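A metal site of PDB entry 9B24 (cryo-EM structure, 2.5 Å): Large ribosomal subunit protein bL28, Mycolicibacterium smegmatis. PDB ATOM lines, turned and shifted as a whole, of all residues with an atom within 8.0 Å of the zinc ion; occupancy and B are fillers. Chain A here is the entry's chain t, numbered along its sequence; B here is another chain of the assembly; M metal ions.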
ATOM      1  N   VAL A   4      -8.132 -23.125 -16.792  1.00  0.00           N
ATOM      2  CA  VAL A   4      -6.691 -22.965 -16.933  1.00  0.00           C
ATOM      3  C   VAL A   4      -6.326 -23.142 -18.401  1.00  0.00           C
ATOM      4  O   VAL A   4      -6.752 -24.108 -19.037  1.00  0.00           O
ATOM      5  CB  VAL A   4      -5.890 -23.974 -16.060  1.00  0.00           C
ATOM      6  CG1 VAL A   4      -4.463 -24.140 -16.591  1.00  0.00           C
ATOM      7  CG2 VAL A   4      -5.820 -23.508 -14.609  1.00  0.00           C
ATOM      8  N   CYS A   5      -5.534 -22.208 -18.931  1.00  0.00           N
ATOM      9  CA  CYS A   5      -4.954 -22.433 -20.250  1.00  0.00           C
ATOM     10  C   CYS A   5      -3.743 -23.341 -20.141  1.00  0.00           C
ATOM     11  O   CYS A   5      -2.970 -23.287 -19.179  1.00  0.00           O
ATOM     12  CB  CYS A   5      -4.568 -21.105 -20.901  1.00  0.00           C
ATOM     13  SG  CYS A   5      -3.279 -20.202 -20.090  1.00  0.00           S
ATOM     14  N   ASP A   6      -3.554 -24.187 -21.147  1.00  0.00           N
ATOM     15  CA  ASP A   6      -2.716 -25.365 -20.992  1.00  0.00           C
ATOM     16  C   ASP A   6      -1.215 -25.105 -20.898  1.00  0.00           C
ATOM     17  O   ASP A   6      -0.471 -26.042 -20.587  1.00  0.00           O
ATOM     18  CB  ASP A   6      -2.949 -26.302 -22.148  1.00  0.00           C
ATOM     19  CG  ASP A   6      -4.286 -26.963 -22.079  1.00  0.00           C
ATOM     20  OD1 ASP A   6      -4.396 -27.990 -21.373  1.00  0.00           O
ATOM     21  OD2 ASP A   6      -5.214 -26.471 -22.728  1.00  0.00           O
ATOM     22  N   ILE A   7      -0.736 -23.897 -21.160  1.00  0.00           N
ATOM     23  CA  ILE A   7       0.715 -23.739 -21.255  1.00  0.00           C
ATOM     24  C   ILE A   7       1.302 -22.884 -20.126  1.00  0.00           C
ATOM     25  O   ILE A   7       2.228 -23.331 -19.424  1.00  0.00           O
ATOM     26  CB  ILE A   7       1.104 -23.208 -22.658  1.00  0.00           C
ATOM     27  CG1 ILE A   7       0.524 -21.840 -22.960  1.00  0.00           C
ATOM     28  CG2 ILE A   7       0.569 -24.081 -23.770  1.00  0.00           C
ATOM     29  CD1 ILE A   7       1.105 -21.302 -24.191  1.00  0.00           C
ATOM     30  N   CYS A   8       0.798 -21.676 -19.914  1.00  0.00           N
ATOM     31  CA  CYS A   8       1.442 -20.854 -18.899  1.00  0.00           C
ATOM     32  C   CYS A   8       0.918 -21.172 -17.508  1.00  0.00           C
ATOM     33  O   CYS A   8       1.366 -20.542 -16.538  1.00  0.00           O
ATOM     34  CB  CYS A   8       1.230 -19.361 -19.154  1.00  0.00           C
ATOM     35  SG  CYS A   8      -0.453 -18.781 -19.289  1.00  0.00           S
ATOM     36  N   GLY A   9      -0.012 -22.109 -17.375  1.00  0.00           N
ATOM     37  CA  GLY A   9      -0.480 -22.527 -16.053  1.00  0.00           C
ATOM     38  C   GLY A   9      -1.184 -21.439 -15.280  1.00  0.00           C
ATOM     39  O   GLY A   9      -0.890 -21.235 -14.108  1.00  0.00           O
ATOM     40  N   LYS A  10      -2.110 -20.724 -15.921  1.00  0.00           N
ATOM     41  CA  LYS A  10      -2.767 -19.602 -15.263  1.00  0.00           C
ATOM     42  C   LYS A  10      -4.102 -20.040 -14.645  1.00  0.00           C
ATOM     43  O   LYS A  10      -4.993 -20.508 -15.350  1.00  0.00           O
ATOM     44  CB  LYS A  10      -2.997 -18.474 -16.264  1.00  0.00           C
ATOM     45  CG  LYS A  10      -3.496 -17.186 -15.650  1.00  0.00           C
ATOM     46  CD  LYS A  10      -4.195 -16.349 -16.694  1.00  0.00           C
ATOM     47  CE  LYS A  10      -3.230 -15.903 -17.773  1.00  0.00           C
ATOM     48  NZ  LYS A  10      -1.952 -15.378 -17.196  1.00  0.00           N
ATOM     49  N   PRO A  31      -9.975 -16.144 -15.913  1.00  0.00           N
ATOM     50  CA  PRO A  31      -9.061 -15.665 -16.951  1.00  0.00           C
ATOM     51  C   PRO A  31      -9.641 -15.839 -18.348  1.00  0.00           C
ATOM     52  O   PRO A  31     -10.443 -16.747 -18.597  1.00  0.00           O
ATOM     53  CB  PRO A  31      -7.819 -16.530 -16.766  1.00  0.00           C
ATOM     54  CG  PRO A  31      -8.333 -17.771 -16.163  1.00  0.00           C
ATOM     55  CD  PRO A  31      -9.485 -17.381 -15.282  1.00  0.00           C
ATOM     56  N   ASN A  32      -9.245 -14.954 -19.250  1.00  0.00           N
ATOM     57  CA  ASN A  32      -9.664 -15.006 -20.642  1.00  0.00           C
ATOM     58  C   ASN A  32      -8.982 -16.174 -21.351  1.00  0.00           C
ATOM     59  O   ASN A  32      -7.866 -16.024 -21.839  1.00  0.00           O
ATOM     60  CB  ASN A  32      -9.305 -13.706 -21.360  1.00  0.00           C
ATOM     61  CG  ASN A  32     -10.409 -13.220 -22.274  1.00  0.00           C
ATOM     62  OD1 ASN A  32     -11.001 -14.015 -22.998  1.00  0.00           O
ATOM     63  ND2 ASN A  32     -10.602 -11.898 -22.343  1.00  0.00           N
ATOM     64  N   ILE A  33      -9.669 -17.305 -21.468  1.00  0.00           N
ATOM     65  CA  ILE A  33      -9.134 -18.426 -22.219  1.00  0.00           C
ATOM     66  C   ILE A  33     -10.151 -18.776 -23.295  1.00  0.00           C
ATOM     67  O   ILE A  33     -11.359 -18.646 -23.082  1.00  0.00           O
ATOM     68  CB  ILE A  33      -8.846 -19.619 -21.303  1.00  0.00           C
ATOM     69  CG1 ILE A  33     -10.136 -20.098 -20.648  1.00  0.00           C
ATOM     70  CG2 ILE A  33      -7.840 -19.212 -20.223  1.00  0.00           C
ATOM     71  CD1 ILE A  33      -9.973 -21.384 -19.935  1.00  0.00           C
ATOM     72  N   ASN A  50      -6.768 -25.176 -25.104  1.00  0.00           N
ATOM     73  CA  ASN A  50      -7.242 -24.045 -24.319  1.00  0.00           C
ATOM     74  C   ASN A  50      -6.073 -23.121 -24.046  1.00  0.00           C
ATOM     75  O   ASN A  50      -5.152 -23.482 -23.300  1.00  0.00           O
ATOM     76  CB  ASN A  50      -7.869 -24.522 -23.006  1.00  0.00           C
ATOM     77  CG  ASN A  50      -9.381 -24.624 -23.068  1.00  0.00           C
ATOM     78  OD1 ASN A  50      -9.964 -24.648 -24.154  1.00  0.00           O
ATOM     79  ND2 ASN A  50     -10.011 -24.673 -21.904  1.00  0.00           N
ATOM     80  N   ALA A  51      -6.096 -21.938 -24.645  1.00  0.00           N
ATOM     81  CA  ALA A  51      -5.029 -20.952 -24.521  1.00  0.00           C
ATOM     82  C   ALA A  51      -5.605 -19.634 -24.048  1.00  0.00           C
ATOM     83  O   ALA A  51      -6.700 -19.238 -24.474  1.00  0.00           O
ATOM     84  CB  ALA A  51      -4.295 -20.747 -25.836  1.00  0.00           C
ATOM     85  N   CYS A  52      -4.887 -18.951 -23.162  1.00  0.00           N
ATOM     86  CA  CYS A  52      -5.418 -17.681 -22.714  1.00  0.00           C
ATOM     87  C   CYS A  52      -5.073 -16.602 -23.733  1.00  0.00           C
ATOM     88  O   CYS A  52      -4.211 -16.768 -24.602  1.00  0.00           O
ATOM     89  CB  CYS A  52      -4.892 -17.281 -21.335  1.00  0.00           C
ATOM     90  SG  CYS A  52      -3.229 -16.564 -21.299  1.00  0.00           S
ATOM     91  N   THR A  53      -5.792 -15.491 -23.624  1.00  0.00           N
ATOM     92  CA  THR A  53      -5.580 -14.378 -24.539  1.00  0.00           C
ATOM     93  C   THR A  53      -4.188 -13.791 -24.394  1.00  0.00           C
ATOM     94  O   THR A  53      -3.581 -13.367 -25.385  1.00  0.00           O
ATOM     95  CB  THR A  53      -6.629 -13.297 -24.307  1.00  0.00           C
ATOM     96  OG1 THR A  53      -7.929 -13.903 -24.280  1.00  0.00           O
ATOM     97  CG2 THR A  53      -6.554 -12.260 -25.389  1.00  0.00           C
ATOM     98  N   SER A  54      -3.666 -13.752 -23.162  1.00  0.00           N
ATOM     99  CA  SER A  54      -2.309 -13.261 -22.967  1.00  0.00           C
ATOM    100  C   SER A  54      -1.314 -14.124 -23.729  1.00  0.00           C
ATOM    101  O   SER A  54      -0.429 -13.608 -24.417  1.00  0.00           O
ATOM    102  CB  SER A  54      -1.948 -13.240 -21.482  1.00  0.00           C
ATOM    103  OG  SER A  54      -1.501 -14.519 -21.052  1.00  0.00           O
ATOM    104  N   CYS A  55      -1.465 -15.439 -23.628  1.00  0.00           N
ATOM    105  CA  CYS A  55      -0.605 -16.356 -24.360  1.00  0.00           C
ATOM    106  C   CYS A  55      -0.749 -16.151 -25.868  1.00  0.00           C
ATOM    107  O   CYS A  55       0.238 -16.181 -26.608  1.00  0.00           O
ATOM    108  CB  CYS A  55      -0.900 -17.809 -24.000  1.00  0.00           C
ATOM    109  SG  CYS A  55      -0.214 -18.399 -22.429  1.00  0.00           S
ATOM    110  N   ILE A  56      -1.983 -15.969 -26.329  1.00  0.00           N
ATOM    111  CA  ILE A  56      -2.214 -15.768 -27.762  1.00  0.00           C
ATOM    112  C   ILE A  56      -1.509 -14.507 -28.239  1.00  0.00           C
ATOM    113  O   ILE A  56      -0.908 -14.476 -29.323  1.00  0.00           O
ATOM    114  CB  ILE A  56      -3.729 -15.730 -28.050  1.00  0.00           C
ATOM    115  CG1 ILE A  56      -4.361 -17.066 -27.682  1.00  0.00           C
ATOM    116  CG2 ILE A  56      -3.998 -15.381 -29.504  1.00  0.00           C
ATOM    117  CD1 ILE A  56      -3.910 -18.230 -28.518  1.00  0.00           C
ATOM    118  N   ALA A  58       1.137 -13.183 -26.773  1.00  0.00           N
ATOM    119  CA  ALA A  58       2.541 -13.575 -26.756  1.00  0.00           C
ATOM    120  C   ALA A  58       2.918 -14.353 -27.996  1.00  0.00           C
ATOM    121  O   ALA A  58       4.095 -14.368 -28.376  1.00  0.00           O
ATOM    122  CB  ALA A  58       2.840 -14.398 -25.500  1.00  0.00           C
ATOM    123  N   LYS A  60       2.878 -17.567 -28.369  1.00  0.00           N
ATOM    124  CA  LYS A  60       3.556 -18.814 -28.050  1.00  0.00           C
ATOM    125  C   LYS A  60       3.024 -19.964 -28.895  1.00  0.00           C
ATOM    126  O   LYS A  60       3.725 -20.966 -29.108  1.00  0.00           O
ATOM    127  CB  LYS A  60       3.410 -19.104 -26.558  1.00  0.00           C
ATOM    128  CG  LYS A  60       4.263 -20.237 -26.028  1.00  0.00           C
ATOM    129  CD  LYS A  60       4.384 -20.169 -24.502  1.00  0.00           C
ATOM    130  CE  LYS A  60       4.614 -18.739 -24.015  1.00  0.00           C
ATOM    131  NZ  LYS A  60       5.792 -18.106 -24.663  1.00  0.00           N
ATOM    132  P     C B 484      -2.242 -13.511 -13.550  1.00  0.00           P
ATOM    133  OP1   C B 484      -2.070 -14.840 -14.187  1.00  0.00           O
ATOM    134  OP2   C B 484      -1.307 -12.414 -13.887  1.00  0.00           O
ATOM    135  O5'   C B 484      -3.726 -12.991 -13.836  1.00  0.00           O
ATOM    136  C5'   C B 484      -4.868 -13.774 -13.517  1.00  0.00           C
ATOM    137  C4'   C B 484      -6.131 -13.056 -13.887  1.00  0.00           C
ATOM    138  O4'   C B 484      -6.353 -11.949 -12.967  1.00  0.00           O
ATOM    139  C3'   C B 484      -6.126 -12.398 -15.265  1.00  0.00           C
ATOM    140  O3'   C B 484      -6.457 -13.295 -16.299  1.00  0.00           O
ATOM    141  C2'   C B 484      -7.108 -11.257 -15.109  1.00  0.00           C
ATOM    142  O2'   C B 484      -8.444 -11.729 -15.184  1.00  0.00           O
ATOM    143  C1'   C B 484      -6.841 -10.822 -13.670  1.00  0.00           C
ATOM    144  N1    C B 484      -5.823  -9.744 -13.571  1.00  0.00           N
ATOM    145  C2    C B 484      -6.142  -8.419 -13.851  1.00  0.00           C
ATOM    146  O2    C B 484      -7.291  -8.130 -14.207  1.00  0.00           O
ATOM    147  N3    C B 484      -5.179  -7.473 -13.735  1.00  0.00           N
ATOM    148  C4    C B 484      -3.951  -7.802 -13.360  1.00  0.00           C
ATOM    149  N4    C B 484      -3.023  -6.844 -13.248  1.00  0.00           N
ATOM    150  C5    C B 484      -3.594  -9.144 -13.060  1.00  0.00           C
ATOM    151  C6    C B 484      -4.552 -10.066 -13.172  1.00  0.00           C
ATOM    152  P     U B 485      -5.768 -13.146 -17.745  1.00  0.00           P
ATOM    153  OP1   U B 485      -6.252 -14.251 -18.606  1.00  0.00           O
ATOM    154  OP2   U B 485      -4.314 -12.946 -17.549  1.00  0.00           O
ATOM    155  O5'   U B 485      -6.366 -11.790 -18.323  1.00  0.00           O
ATOM    156  C5'   U B 485      -7.753 -11.658 -18.600  1.00  0.00           C
ATOM    157  C4'   U B 485      -8.135 -10.215 -18.825  1.00  0.00           C
ATOM    158  O4'   U B 485      -7.754  -9.425 -17.680  1.00  0.00           O
ATOM    159  C3'   U B 485      -7.458  -9.528 -20.002  1.00  0.00           C
ATOM    160  O3'   U B 485      -8.115  -9.807 -21.229  1.00  0.00           O
ATOM    161  C2'   U B 485      -7.514  -8.057 -19.618  1.00  0.00           C
ATOM    162  O2'   U B 485      -8.771  -7.497 -19.971  1.00  0.00           O
ATOM    163  C1'   U B 485      -7.421  -8.116 -18.085  1.00  0.00           C
ATOM    164  N1    U B 485      -6.068  -7.775 -17.587  1.00  0.00           N
ATOM    165  C2    U B 485      -5.759  -6.430 -17.523  1.00  0.00           C
ATOM    166  O2    U B 485      -6.538  -5.563 -17.874  1.00  0.00           O
ATOM    167  N3    U B 485      -4.514  -6.134 -17.046  1.00  0.00           N
ATOM    168  C4    U B 485      -3.571  -7.036 -16.624  1.00  0.00           C
ATOM    169  O4    U B 485      -2.481  -6.617 -16.218  1.00  0.00           O
ATOM    170  C5    U B 485      -3.955  -8.407 -16.710  1.00  0.00           C
ATOM    171  C6    U B 485      -5.172  -8.730 -17.169  1.00  0.00           C
HETATM  172 ZN    ZN M   1      -2.007 -18.469 -20.962  1.00  0.00          ZN
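Merely in contact with the zinc ion: Ser 54 (3.98 Å).
Of the 21 residues printed, 5 come within 4 Å of the zinc ion.
SG of Cys 52 sits close to OG of Ser 54 (2.7 Å).
The backbone carbonyl oxygen (O) of Cys 55 sits at hydrogen-bond distance from the backbone NH (N) of Lys 60 (3.5 Å).
The zinc ion is bound by SG of Cys 52 (2.3 Å), SG of Cys 8 (2.3 Å), SG of Cys 55 (2.3 Å) and SG of Cys 5 (2.3 Å).
The zinc ion has four donor atoms within binding distance.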
